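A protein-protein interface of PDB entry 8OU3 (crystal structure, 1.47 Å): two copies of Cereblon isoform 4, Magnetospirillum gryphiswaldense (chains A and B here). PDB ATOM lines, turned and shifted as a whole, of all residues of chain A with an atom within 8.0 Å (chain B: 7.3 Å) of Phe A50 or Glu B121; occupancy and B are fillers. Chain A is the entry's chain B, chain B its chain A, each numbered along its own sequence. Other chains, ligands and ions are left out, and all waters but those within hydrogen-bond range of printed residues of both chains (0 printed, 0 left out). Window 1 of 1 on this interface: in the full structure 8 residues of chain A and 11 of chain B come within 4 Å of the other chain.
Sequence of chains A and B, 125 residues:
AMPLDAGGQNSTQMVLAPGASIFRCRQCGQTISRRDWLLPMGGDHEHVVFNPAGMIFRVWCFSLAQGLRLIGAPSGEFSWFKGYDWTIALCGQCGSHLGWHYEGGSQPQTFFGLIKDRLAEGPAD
Printed residues of chain B within 4 Å of Val A49: Glu B121 (3.1 Å). Of chain B, only Ile B22 (3.7 Å), Arg B24 (3.5 Å), Ala B120 (3.4 Å), Glu B121 (3.0 Å), Gly B122 (3.2 Å) and Pro B123 (3.2 Å) come within 4 Å of Phe A50. Printed residues of chain B within 4 Å of Trp A80: Gly B19 and Ala B20. Of the printed residues of chain A, Gly B19 touches Phe A78, Ser A79 and Trp A80. Asp B36 touches none of the printed residues of chain A. Of the printed residues of chain A, Leu B119 touches Val A48. Of chain A, only Val A48 and Phe A50 come within 4 Å of Ala B120. Of the printed residues of chain A, Glu B121 touches Val A48, Val A49 and Phe A50. The nearest residue of chain A that does not touch Glu B121 is Trp A80 (4.1 Å).
No position is printed for both chains. Of the 15 pairs that touch across the chains among the printed residues, none has its exchanged pair printed and touching as well.
O of Val A48 sits at hydrogen-bond distance from N of Glu B121, at 2.9 Å. O of Ser A79 is in hydrogen-bond range of N of Gly B19 (3.1 Å). The backbone NH (N) of Phe A50 is in hydrogen-bond range of the backbone carbonyl oxygen (O) of Glu B121 (3.0 Å).
Of the 20 printed residues of chain B, 9 touch a printed residue of chain A. Printed residues of chain B that touch a printed residue of chain A: Gly B19, Ala B20, Ile B22, Arg B24, Leu B119, Ala B120, Glu B121, Gly B122 and Pro B123. Hydrophobic or aromatic side chains of chain B within 4 Å of the printed part of chain A: Ala B20, Ala B120 and Pro B123. Of the 17 printed residues of chain A, 6 touch a printed residue of chain B. Among the printed residues, 15 pairs touch across the chains.
Among the printed residues, merely in contact across the chains: Val A49 with Glu B121, Phe A50 with Pro B123, Phe A50 with Gly B122, Trp A80 with Gly B19, Val A48 with Ala B120, Val A48 with Leu B119, Phe A78 with Gly B19, Phe A50 with Ala B120, Phe A50 with Arg B24, Phe A50 with Ile B22, Trp A80 with Ala B20 and Phe A78 with Pro B123.
N of Ser B21 is in hydrogen-bond range of O of Gly B122, 3.0 Å away. The backbone carbonyl oxygen of Phe A81 sits at hydrogen-bond distance from the side-chain hydroxyl of Ser A79 (3.1 Å). The backbone carbonyl oxygen of Val A49 is in hydrogen-bond range of the backbone NH of Phe A57 (2.9 Å). The side-chain carboxylate of Glu B121 is in salt-bridge range of the guanidinium group of Arg B35, 2.5 Å away. The backbone NH (N) of Ile B22 lies within hydrogen-bond range of the backbone carbonyl oxygen (O) of Gly B122 (2.9 Å). The guanidinium group (NH1) of Arg B24 lies within hydrogen-bond range of the backbone carbonyl oxygen (O) of Gly B29 (2.9 Å).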
ATOM      1  N   HIS A  47      19.944   3.111 -17.155  1.00  0.00           N
ATOM      2  CA  HIS A  47      19.797   2.036 -16.179  1.00  0.00           C
ATOM      3  C   HIS A  47      19.230   0.803 -16.876  1.00  0.00           C
ATOM      4  O   HIS A  47      18.100   0.842 -17.393  1.00  0.00           O
ATOM      5  CB  HIS A  47      18.855   2.461 -15.051  1.00  0.00           C
ATOM      6  CG  HIS A  47      19.330   3.688 -14.349  1.00  0.00           C
ATOM      7  ND1 HIS A  47      19.897   3.562 -13.097  1.00  0.00           N
ATOM      8  CD2 HIS A  47      19.431   4.985 -14.688  1.00  0.00           C
ATOM      9  CE1 HIS A  47      20.311   4.756 -12.696  1.00  0.00           C
ATOM     10  NE2 HIS A  47      20.015   5.618 -13.618  1.00  0.00           N
ATOM     11  N   VAL A  48      20.019  -0.269 -16.849  1.00  0.00           N
ATOM     12  CA  VAL A  48      19.543  -1.569 -17.287  1.00  0.00           C
ATOM     13  C   VAL A  48      18.949  -2.280 -16.078  1.00  0.00           C
ATOM     14  O   VAL A  48      19.625  -2.492 -15.074  1.00  0.00           O
ATOM     15  CB  VAL A  48      20.614  -2.402 -17.980  1.00  0.00           C
ATOM     16  CG1 VAL A  48      20.101  -3.727 -18.495  1.00  0.00           C
ATOM     17  CG2 VAL A  48      21.297  -1.630 -19.136  1.00  0.00           C
ATOM     18  N   VAL A  49      17.677  -2.660 -16.210  1.00  0.00           N
ATOM     19  CA  VAL A  49      16.856  -3.110 -15.070  1.00  0.00           C
ATOM     20  C   VAL A  49      16.061  -4.366 -15.470  1.00  0.00           C
ATOM     21  O   VAL A  49      15.841  -4.631 -16.656  1.00  0.00           O
ATOM     22  CB  VAL A  49      15.940  -1.981 -14.591  1.00  0.00           C
ATOM     23  CG1 VAL A  49      16.722  -0.797 -14.007  1.00  0.00           C
ATOM     24  CG2 VAL A  49      15.002  -1.516 -15.687  1.00  0.00           C
ATOM     25  N   PHE A  50      15.548  -5.110 -14.462  1.00  0.00           N
ATOM     26  CA  PHE A  50      14.604  -6.188 -14.762  1.00  0.00           C
ATOM     27  C   PHE A  50      13.442  -6.126 -13.757  1.00  0.00           C
ATOM     28  O   PHE A  50      13.621  -5.668 -12.612  1.00  0.00           O
ATOM     29  CB  PHE A  50      15.266  -7.548 -14.783  1.00  0.00           C
ATOM     30  CG  PHE A  50      15.841  -8.002 -13.454  1.00  0.00           C
ATOM     31  CD1 PHE A  50      15.052  -8.657 -12.514  1.00  0.00           C
ATOM     32  CD2 PHE A  50      17.169  -7.762 -13.113  1.00  0.00           C
ATOM     33  CE1 PHE A  50      15.572  -9.077 -11.311  1.00  0.00           C
ATOM     34  CE2 PHE A  50      17.680  -8.155 -11.883  1.00  0.00           C
ATOM     35  CZ  PHE A  50      16.881  -8.796 -10.970  1.00  0.00           C
ATOM     36  N   ASN A  51      12.259  -6.470 -14.254  1.00  0.00           N
ATOM     37  CA  ASN A  51      11.074  -6.498 -13.384  1.00  0.00           C
ATOM     38  C   ASN A  51      10.902  -7.888 -12.765  1.00  0.00           C
ATOM     39  O   ASN A  51      11.666  -8.857 -12.916  1.00  0.00           O
ATOM     40  CB  ASN A  51       9.873  -6.027 -14.201  1.00  0.00           C
ATOM     41  CG  ASN A  51       9.386  -6.984 -15.254  1.00  0.00           C
ATOM     42  OD1 ASN A  51       9.720  -8.168 -15.277  1.00  0.00           O
ATOM     43  ND2 ASN A  51       8.482  -6.490 -16.082  1.00  0.00           N
ATOM     44  N   PRO A  52       9.872  -8.079 -11.877  1.00  0.00           N
ATOM     45  CA  PRO A  52       9.688  -9.356 -11.233  1.00  0.00           C
ATOM     46  C   PRO A  52       9.336 -10.546 -12.137  1.00  0.00           C
ATOM     47  O   PRO A  52       9.477 -11.661 -11.717  1.00  0.00           O
ATOM     48  CB  PRO A  52       8.539  -9.119 -10.231  1.00  0.00           C
ATOM     49  CG  PRO A  52       8.564  -7.638 -10.003  1.00  0.00           C
ATOM     50  CD  PRO A  52       9.041  -7.004 -11.309  1.00  0.00           C
ATOM     51  N   ALA A  53       8.817 -10.249 -13.336  1.00  0.00           N
ATOM     52  CA  ALA A  53       8.564 -11.285 -14.322  1.00  0.00           C
ATOM     53  C   ALA A  53       9.821 -11.577 -15.153  1.00  0.00           C
ATOM     54  O   ALA A  53       9.770 -12.493 -15.973  1.00  0.00           O
ATOM     55  CB  ALA A  53       7.420 -10.850 -15.235  1.00  0.00           C
ATOM     56  N   GLY A  54      10.935 -10.962 -14.785  1.00  0.00           N
ATOM     57  CA  GLY A  54      12.229 -11.214 -15.428  1.00  0.00           C
ATOM     58  C   GLY A  54      12.376 -10.528 -16.785  1.00  0.00           C
ATOM     59  O   GLY A  54      13.349 -10.854 -17.508  1.00  0.00           O
ATOM     60  N   MET A  55      11.507  -9.585 -17.143  1.00  0.00           N
ATOM     61  CA  MET A  55      11.700  -8.823 -18.373  1.00  0.00           C
ATOM     62  C   MET A  55      12.801  -7.797 -18.129  1.00  0.00           C
ATOM     63  O   MET A  55      12.804  -7.092 -17.121  1.00  0.00           O
ATOM     64  CB  MET A  55      10.401  -8.148 -18.820  1.00  0.00           C
ATOM     65  CG  MET A  55       9.314  -9.104 -19.119  1.00  0.00           C
ATOM     66  SD  MET A  55       9.614  -9.971 -20.698  1.00  0.00           S
ATOM     67  CE  MET A  55      10.154 -11.527 -20.039  1.00  0.00           C
ATOM     68  N   ILE A  56      13.755  -7.667 -19.097  1.00  0.00           N
ATOM     69  CA  ILE A  56      14.848  -6.698 -19.028  1.00  0.00           C
ATOM     70  C   ILE A  56      14.562  -5.485 -19.889  1.00  0.00           C
ATOM     71  O   ILE A  56      14.094  -5.601 -21.044  1.00  0.00           O
ATOM     72  CB  ILE A  56      16.159  -7.386 -19.433  1.00  0.00           C
ATOM     73  CG1 ILE A  56      16.524  -8.492 -18.441  1.00  0.00           C
ATOM     74  CG2 ILE A  56      17.296  -6.380 -19.602  1.00  0.00           C
ATOM     75  CD1 ILE A  56      17.619  -9.427 -18.834  1.00  0.00           C
ATOM     76  N   PHE A  57      14.859  -4.299 -19.323  1.00  0.00           N
ATOM     77  CA  PHE A  57      14.654  -3.044 -20.017  1.00  0.00           C
ATOM     78  C   PHE A  57      15.892  -2.169 -19.877  1.00  0.00           C
ATOM     79  O   PHE A  57      16.544  -2.170 -18.830  1.00  0.00           O
ATOM     80  CB  PHE A  57      13.482  -2.221 -19.452  1.00  0.00           C
ATOM     81  CG  PHE A  57      12.166  -2.972 -19.436  1.00  0.00           C
ATOM     82  CD1 PHE A  57      11.303  -2.871 -20.520  1.00  0.00           C
ATOM     83  CD2 PHE A  57      11.753  -3.734 -18.350  1.00  0.00           C
ATOM     84  CE1 PHE A  57      10.103  -3.564 -20.547  1.00  0.00           C
ATOM     85  CE2 PHE A  57      10.559  -4.429 -18.387  1.00  0.00           C
ATOM     86  CZ  PHE A  57       9.725  -4.325 -19.463  1.00  0.00           C
ATOM     87  N   ARG A  58      16.205  -1.413 -20.940  1.00  0.00           N
ATOM     88  CA  ARG A  58      17.242  -0.409 -20.889  1.00  0.00           C
ATOM     89  C   ARG A  58      16.548   0.940 -20.861  1.00  0.00           C
ATOM     90  O   ARG A  58      15.966   1.389 -21.874  1.00  0.00           O
ATOM     91  CB  ARG A  58      18.257  -0.574 -22.038  1.00  0.00           C
ATOM     92  CG  ARG A  58      19.366   0.467 -22.051  1.00  0.00           C
ATOM     93  CD  ARG A  58      20.438   0.109 -23.041  1.00  0.00           C
ATOM     94  NE  ARG A  58      19.903   0.098 -24.401  1.00  0.00           N
ATOM     95  CZ  ARG A  58      20.181   1.021 -25.322  1.00  0.00           C
ATOM     96  NH1 ARG A  58      20.885   2.084 -24.988  1.00  0.00           N
ATOM     97  NH2 ARG A  58      19.590   0.951 -26.509  1.00  0.00           N
ATOM     98  N   VAL A  59      16.570   1.582 -19.693  1.00  0.00           N
ATOM     99  CA  VAL A  59      15.796   2.765 -19.396  1.00  0.00           C
ATOM    100  C   VAL A  59      16.727   3.972 -19.356  1.00  0.00           C
ATOM    101  O   VAL A  59      17.826   3.883 -18.815  1.00  0.00           O
ATOM    102  CB  VAL A  59      15.105   2.557 -18.028  1.00  0.00           C
ATOM    103  CG1 VAL A  59      14.498   3.808 -17.488  1.00  0.00           C
ATOM    104  CG2 VAL A  59      14.092   1.396 -18.111  1.00  0.00           C
ATOM    105  N   PHE A  78       8.551  -2.859  -5.926  1.00  0.00           N
ATOM    106  CA  PHE A  78       9.646  -3.189  -6.825  1.00  0.00           C
ATOM    107  C   PHE A  78      10.157  -1.968  -7.581  1.00  0.00           C
ATOM    108  O   PHE A  78      10.771  -2.084  -8.653  1.00  0.00           O
ATOM    109  CB  PHE A  78       9.232  -4.250  -7.848  1.00  0.00           C
ATOM    110  CG  PHE A  78       8.514  -5.450  -7.293  1.00  0.00           C
ATOM    111  CD1 PHE A  78       9.184  -6.332  -6.484  1.00  0.00           C
ATOM    112  CD2 PHE A  78       7.174  -5.681  -7.603  1.00  0.00           C
ATOM    113  CE1 PHE A  78       8.526  -7.442  -5.978  1.00  0.00           C
ATOM    114  CE2 PHE A  78       6.522  -6.787  -7.089  1.00  0.00           C
ATOM    115  CZ  PHE A  78       7.206  -7.654  -6.279  1.00  0.00           C
ATOM    116  N   SER A  79       9.987  -0.761  -7.017  1.00  0.00           N
ATOM    117  CA  SER A  79      10.503   0.393  -7.726  1.00  0.00           C
ATOM    118  C   SER A  79      12.005   0.264  -7.960  1.00  0.00           C
ATOM    119  O   SER A  79      12.763   0.000  -7.010  1.00  0.00           O
ATOM    120  CB  SER A  79      10.241   1.657  -6.935  1.00  0.00           C
ATOM    121  OG  SER A  79      10.691   2.758  -7.689  1.00  0.00           O
ATOM    122  N   TRP A  80      12.436   0.609  -9.184  1.00  0.00           N
ATOM    123  CA  TRP A  80      13.855   0.579  -9.517  1.00  0.00           C
ATOM    124  C   TRP A  80      14.610   1.754  -8.883  1.00  0.00           C
ATOM    125  O   TRP A  80      15.846   1.781  -8.900  1.00  0.00           O
ATOM    126  CB  TRP A  80      14.059   0.539 -11.030  1.00  0.00           C
ATOM    127  CG  TRP A  80      13.592  -0.721 -11.694  1.00  0.00           C
ATOM    128  CD1 TRP A  80      13.810  -1.987 -11.257  1.00  0.00           C
ATOM    129  CD2 TRP A  80      12.811  -0.837 -12.889  1.00  0.00           C
ATOM    130  NE1 TRP A  80      13.251  -2.873 -12.138  1.00  0.00           N
ATOM    131  CE2 TRP A  80      12.642  -2.217 -13.143  1.00  0.00           C
ATOM    132  CE3 TRP A  80      12.297   0.079 -13.817  1.00  0.00           C
ATOM    133  CZ2 TRP A  80      11.925  -2.696 -14.246  1.00  0.00           C
ATOM    134  CZ3 TRP A  80      11.599  -0.396 -14.909  1.00  0.00           C
ATOM    135  CH2 TRP A  80      11.446  -1.769 -15.140  1.00  0.00           C
ATOM    136  N   PHE A  81      13.888   2.763  -8.391  1.00  0.00           N
ATOM    137  CA  PHE A  81      14.470   3.974  -7.856  1.00  0.00           C
ATOM    138  C   PHE A  81      13.964   4.169  -6.438  1.00  0.00           C
ATOM    139  O   PHE A  81      12.793   4.498  -6.221  1.00  0.00           O
ATOM    140  CB  PHE A  81      14.187   5.163  -8.794  1.00  0.00           C
ATOM    141  CG  PHE A  81      14.719   4.968 -10.192  1.00  0.00           C
ATOM    142  CD1 PHE A  81      16.051   5.207 -10.498  1.00  0.00           C
ATOM    143  CD2 PHE A  81      13.871   4.550 -11.209  1.00  0.00           C
ATOM    144  CE1 PHE A  81      16.513   4.939 -11.782  1.00  0.00           C
ATOM    145  CE2 PHE A  81      14.333   4.341 -12.497  1.00  0.00           C
ATOM    146  CZ  PHE A  81      15.659   4.525 -12.770  1.00  0.00           C
ATOM    147  N   GLY B  19      13.410  -2.700  -5.629  1.00  0.00           N
ATOM    148  CA  GLY B  19      13.608  -3.059  -7.035  1.00  0.00           C
ATOM    149  C   GLY B  19      15.054  -2.922  -7.501  1.00  0.00           C
ATOM    150  O   GLY B  19      15.382  -3.158  -8.673  1.00  0.00           O
ATOM    151  N   ALA B  20      15.955  -2.554  -6.588  1.00  0.00           N
ATOM    152  CA  ALA B  20      17.352  -2.373  -6.948  1.00  0.00           C
ATOM    153  C   ALA B  20      18.185  -3.117  -5.915  1.00  0.00           C
ATOM    154  O   ALA B  20      18.740  -2.493  -5.009  1.00  0.00           O
ATOM    155  CB  ALA B  20      17.701  -0.901  -6.979  1.00  0.00           C
ATOM    156  N   SER B  21      18.112  -4.439  -5.937  1.00  0.00           N
ATOM    157  CA  SER B  21      18.854  -5.175  -4.939  1.00  0.00           C
ATOM    158  C   SER B  21      19.796  -6.185  -5.581  1.00  0.00           C
ATOM    159  O   SER B  21      20.866  -6.395  -4.992  1.00  0.00           O
ATOM    160  CB  SER B  21      17.977  -5.773  -3.842  1.00  0.00           C
ATOM    161  OG  SER B  21      17.638  -7.111  -4.136  1.00  0.00           O
ATOM    162  N   ILE B  22      19.439  -6.806  -6.716  1.00  0.00           N
ATOM    163  CA  ILE B  22      20.193  -7.912  -7.287  1.00  0.00           C
ATOM    164  C   ILE B  22      20.704  -7.474  -8.671  1.00  0.00           C
ATOM    165  O   ILE B  22      19.974  -6.791  -9.392  1.00  0.00           O
ATOM    166  CB  ILE B  22      19.336  -9.194  -7.389  1.00  0.00           C
ATOM    167  CG1 ILE B  22      19.046  -9.770  -5.989  1.00  0.00           C
ATOM    168  CG2 ILE B  22      19.945 -10.255  -8.269  1.00  0.00           C
ATOM    169  N   PHE B  23      21.949  -7.805  -9.017  1.00  0.00           N
ATOM    170  CA  PHE B  23      22.454  -7.666 -10.363  1.00  0.00           C
ATOM    171  C   PHE B  23      22.504  -9.034 -11.028  1.00  0.00           C
ATOM    172  O   PHE B  23      23.052  -9.989 -10.491  1.00  0.00           O
ATOM    173  CB  PHE B  23      23.857  -7.056 -10.366  1.00  0.00           C
ATOM    174  CG  PHE B  23      23.903  -5.615  -9.951  1.00  0.00           C
ATOM    175  CD1 PHE B  23      23.636  -4.591 -10.847  1.00  0.00           C
ATOM    176  CD2 PHE B  23      24.184  -5.263  -8.636  1.00  0.00           C
ATOM    177  CE1 PHE B  23      23.642  -3.267 -10.434  1.00  0.00           C
ATOM    178  CE2 PHE B  23      24.211  -3.941  -8.231  1.00  0.00           C
ATOM    179  CZ  PHE B  23      23.914  -2.947  -9.118  1.00  0.00           C
ATOM    180  N   ARG B  24      21.970  -9.054 -12.252  1.00  0.00           N
ATOM    181  CA  ARG B  24      21.990 -10.278 -13.076  1.00  0.00           C
ATOM    182  C   ARG B  24      22.668  -9.992 -14.424  1.00  0.00           C
ATOM    183  O   ARG B  24      22.755  -8.835 -14.788  1.00  0.00           O
ATOM    184  CB  ARG B  24      20.559 -10.744 -13.352  1.00  0.00           C
ATOM    185  CG  ARG B  24      19.795 -11.180 -12.113  1.00  0.00           C
ATOM    186  CD  ARG B  24      18.400 -11.670 -12.454  1.00  0.00           C
ATOM    187  NE  ARG B  24      17.706 -12.209 -11.295  1.00  0.00           N
ATOM    188  CZ  ARG B  24      18.065 -13.311 -10.652  1.00  0.00           C
ATOM    189  NH1 ARG B  24      18.815 -14.216 -11.251  1.00  0.00           N
ATOM    190  NH2 ARG B  24      17.660 -13.511  -9.411  1.00  0.00           N
ATOM    191  N   CYS B  25      23.144 -11.032 -15.105  1.00  0.00           N
ATOM    192  CA  CYS B  25      23.679 -10.894 -16.451  1.00  0.00           C
ATOM    193  C   CYS B  25      22.587 -10.348 -17.376  1.00  0.00           C
ATOM    194  O   CYS B  25      21.482 -10.878 -17.395  1.00  0.00           O
ATOM    195  CB  CYS B  25      24.147 -12.247 -16.954  1.00  0.00           C
ATOM    196  SG  CYS B  25      24.751 -12.154 -18.661  1.00  0.00           S
ATOM    197  N   GLY B  29      20.257 -13.463 -17.503  1.00  0.00           N
ATOM    198  CA  GLY B  29      19.574 -13.527 -16.233  1.00  0.00           C
ATOM    199  C   GLY B  29      20.311 -14.225 -15.090  1.00  0.00           C
ATOM    200  O   GLY B  29      19.799 -14.225 -13.949  1.00  0.00           O
ATOM    201  N   ARG B  34      25.031  -8.136  -5.865  1.00  0.00           N
ATOM    202  CA  ARG B  34      24.006  -7.459  -5.097  1.00  0.00           C
ATOM    203  C   ARG B  34      24.468  -6.032  -4.853  1.00  0.00           C
ATOM    204  O   ARG B  34      25.678  -5.787  -4.683  1.00  0.00           O
ATOM    205  CB  ARG B  34      23.740  -8.136  -3.742  1.00  0.00           C
ATOM    206  CG  ARG B  34      23.427  -9.627  -3.828  1.00  0.00           C
ATOM    207  CD  ARG B  34      22.991 -10.171  -2.461  1.00  0.00           C
ATOM    208  NE  ARG B  34      21.810  -9.458  -1.998  1.00  0.00           N
ATOM    209  CZ  ARG B  34      20.564  -9.900  -2.105  1.00  0.00           C
ATOM    210  NH1 ARG B  34      20.320 -11.067  -2.668  1.00  0.00           N
ATOM    211  NH2 ARG B  34      19.559  -9.178  -1.638  1.00  0.00           N
ATOM    212  N   ARG B  35      23.524  -5.097  -4.795  1.00  0.00           N
ATOM    213  CA  ARG B  35      23.858  -3.731  -4.461  1.00  0.00           C
ATOM    214  C   ARG B  35      24.591  -3.646  -3.112  1.00  0.00           C
ATOM    215  O   ARG B  35      25.479  -2.807  -2.937  1.00  0.00           O
ATOM    216  CB  ARG B  35      22.600  -2.873  -4.542  1.00  0.00           C
ATOM    217  CG  ARG B  35      22.816  -1.418  -4.152  1.00  0.00           C
ATOM    218  CD  ARG B  35      21.707  -0.501  -4.648  1.00  0.00           C
ATOM    219  NE  ARG B  35      21.766  -0.240  -6.094  1.00  0.00           N
ATOM    220  CZ  ARG B  35      22.522   0.681  -6.690  1.00  0.00           C
ATOM    221  NH1 ARG B  35      23.420   1.378  -6.011  1.00  0.00           N
ATOM    222  NH2 ARG B  35      22.374   0.910  -7.980  1.00  0.00           N
ATOM    223  N   ASP B  36      24.175  -4.481  -2.156  1.00  0.00           N
ATOM    224  CA  ASP B  36      24.751  -4.455  -0.821  1.00  0.00           C
ATOM    225  C   ASP B  36      26.248  -4.776  -0.849  1.00  0.00           C
ATOM    226  O   ASP B  36      26.924  -4.512   0.150  1.00  0.00           O
ATOM    227  CB  ASP B  36      24.036  -5.446   0.107  1.00  0.00           C
ATOM    228  CG  ASP B  36      22.668  -4.994   0.576  1.00  0.00           C
ATOM    229  OD1 ASP B  36      22.375  -3.798   0.477  1.00  0.00           O
ATOM    230  OD2 ASP B  36      21.942  -5.835   1.119  1.00  0.00           O
ATOM    231  N   LEU B  38      28.450  -3.677  -3.185  1.00  0.00           N
ATOM    232  CA  LEU B  38      29.297  -2.662  -3.810  1.00  0.00           C
ATOM    233  C   LEU B  38      30.436  -2.282  -2.860  1.00  0.00           C
ATOM    234  O   LEU B  38      30.265  -2.214  -1.642  1.00  0.00           O
ATOM    235  CB  LEU B  38      28.452  -1.442  -4.176  1.00  0.00           C
ATOM    236  CG  LEU B  38      27.595  -1.581  -5.423  1.00  0.00           C
ATOM    237  CD1 LEU B  38      26.568  -0.475  -5.472  1.00  0.00           C
ATOM    238  CD2 LEU B  38      28.472  -1.568  -6.665  1.00  0.00           C
ATOM    239  N   TRP B  60      32.058  -1.105 -12.012  1.00  0.00           N
ATOM    240  CA  TRP B  60      31.598  -1.069 -10.627  1.00  0.00           C
ATOM    241  C   TRP B  60      32.381  -2.140  -9.872  1.00  0.00           C
ATOM    242  O   TRP B  60      32.425  -3.284 -10.321  1.00  0.00           O
ATOM    243  CB  TRP B  60      30.078  -1.256 -10.545  1.00  0.00           C
ATOM    244  CG  TRP B  60      29.331   0.002 -10.891  1.00  0.00           C
ATOM    245  CD1 TRP B  60      29.834   1.068 -11.585  1.00  0.00           C
ATOM    246  CD2 TRP B  60      28.003   0.395 -10.503  1.00  0.00           C
ATOM    247  NE1 TRP B  60      28.898   2.063 -11.700  1.00  0.00           N
ATOM    248  CE2 TRP B  60      27.792   1.701 -10.993  1.00  0.00           C
ATOM    249  CE3 TRP B  60      27.006  -0.201  -9.729  1.00  0.00           C
ATOM    250  CZ2 TRP B  60      26.597   2.397 -10.797  1.00  0.00           C
ATOM    251  CZ3 TRP B  60      25.841   0.497  -9.494  1.00  0.00           C
ATOM    252  CH2 TRP B  60      25.626   1.763 -10.055  1.00  0.00           C
ATOM    253  N   LYS B 116      29.210  -2.207 -15.757  1.00  0.00           N
ATOM    254  CA  LYS B 116      27.882  -1.865 -15.279  1.00  0.00           C
ATOM    255  C   LYS B 116      26.822  -2.097 -16.356  1.00  0.00           C
ATOM    256  O   LYS B 116      25.739  -2.592 -16.050  1.00  0.00           O
ATOM    257  CB  LYS B 116      27.878  -0.415 -14.787  1.00  0.00           C
ATOM    258  N   LEU B 119      25.196  -5.660 -16.906  1.00  0.00           N
ATOM    259  CA  LEU B 119      24.363  -6.206 -15.831  1.00  0.00           C
ATOM    260  C   LEU B 119      22.973  -5.585 -15.944  1.00  0.00           C
ATOM    261  O   LEU B 119      22.823  -4.435 -16.391  1.00  0.00           O
ATOM    262  CB  LEU B 119      25.004  -5.889 -14.475  1.00  0.00           C
ATOM    263  CG  LEU B 119      26.445  -6.356 -14.258  1.00  0.00           C
ATOM    264  CD1 LEU B 119      26.956  -5.854 -12.914  1.00  0.00           C
ATOM    265  CD2 LEU B 119      26.527  -7.873 -14.333  1.00  0.00           C
ATOM    266  N   ALA B 120      21.973  -6.279 -15.388  1.00  0.00           N
ATOM    267  CA  ALA B 120      20.652  -5.727 -15.157  1.00  0.00           C
ATOM    268  C   ALA B 120      20.326  -5.751 -13.669  1.00  0.00           C
ATOM    269  O   ALA B 120      20.617  -6.753 -13.023  1.00  0.00           O
ATOM    270  CB  ALA B 120      19.618  -6.498 -15.893  1.00  0.00           C
ATOM    271  N   GLU B 121      19.843  -4.631 -13.149  1.00  0.00           N
ATOM    272  CA  GLU B 121      19.558  -4.527 -11.731  1.00  0.00           C
ATOM    273  C   GLU B 121      18.057  -4.669 -11.495  1.00  0.00           C
ATOM    274  O   GLU B 121      17.234  -4.100 -12.205  1.00  0.00           O
ATOM    275  CB  GLU B 121      20.120  -3.192 -11.237  1.00  0.00           C
ATOM    276  CG  GLU B 121      20.210  -3.142  -9.712  1.00  0.00           C
ATOM    277  CD  GLU B 121      20.750  -1.837  -9.141  1.00  0.00           C
ATOM    278  OE1 GLU B 121      21.043  -0.910  -9.942  1.00  0.00           O
ATOM    279  OE2 GLU B 121      20.850  -1.747  -7.901  1.00  0.00           O
ATOM    280  N   GLY B 122      17.659  -5.313 -10.387  1.00  0.00           N
ATOM    281  CA  GLY B 122      16.266  -5.562 -10.169  1.00  0.00           C
ATOM    282  C   GLY B 122      16.004  -6.174  -8.787  1.00  0.00           C
ATOM    283  O   GLY B 122      16.887  -6.287  -7.935  1.00  0.00           O
ATOM    284  N   PRO B 123      14.772  -6.593  -8.581  1.00  0.00           N
ATOM    285  CA  PRO B 123      14.342  -7.078  -7.267  1.00  0.00           C
ATOM    286  C   PRO B 123      14.932  -8.442  -6.918  1.00  0.00           C
ATOM    287  O   PRO B 123      15.255  -9.220  -7.793  1.00  0.00           O
ATOM    288  CB  PRO B 123      12.834  -7.148  -7.374  1.00  0.00           C
ATOM    289  CG  PRO B 123      12.535  -7.287  -8.848  1.00  0.00           C
ATOM    290  CD  PRO B 123      13.653  -6.538  -9.539  1.00  0.00           C
ATOM    291  N   ALA B 124      15.001  -8.734  -5.608  1.00  0.00           N
ATOM    292  CA  ALA B 124      15.580  -9.979  -5.116  1.00  0.00           C
ATOM    293  C   ALA B 124      14.795 -11.181  -5.659  1.00  0.00           C
ATOM    294  O   ALA B 124      13.572 -11.055  -5.736  1.00  0.00           O
ATOM    295  CB  ALA B 124      15.591  -9.983  -3.615  1.00  0.00           C
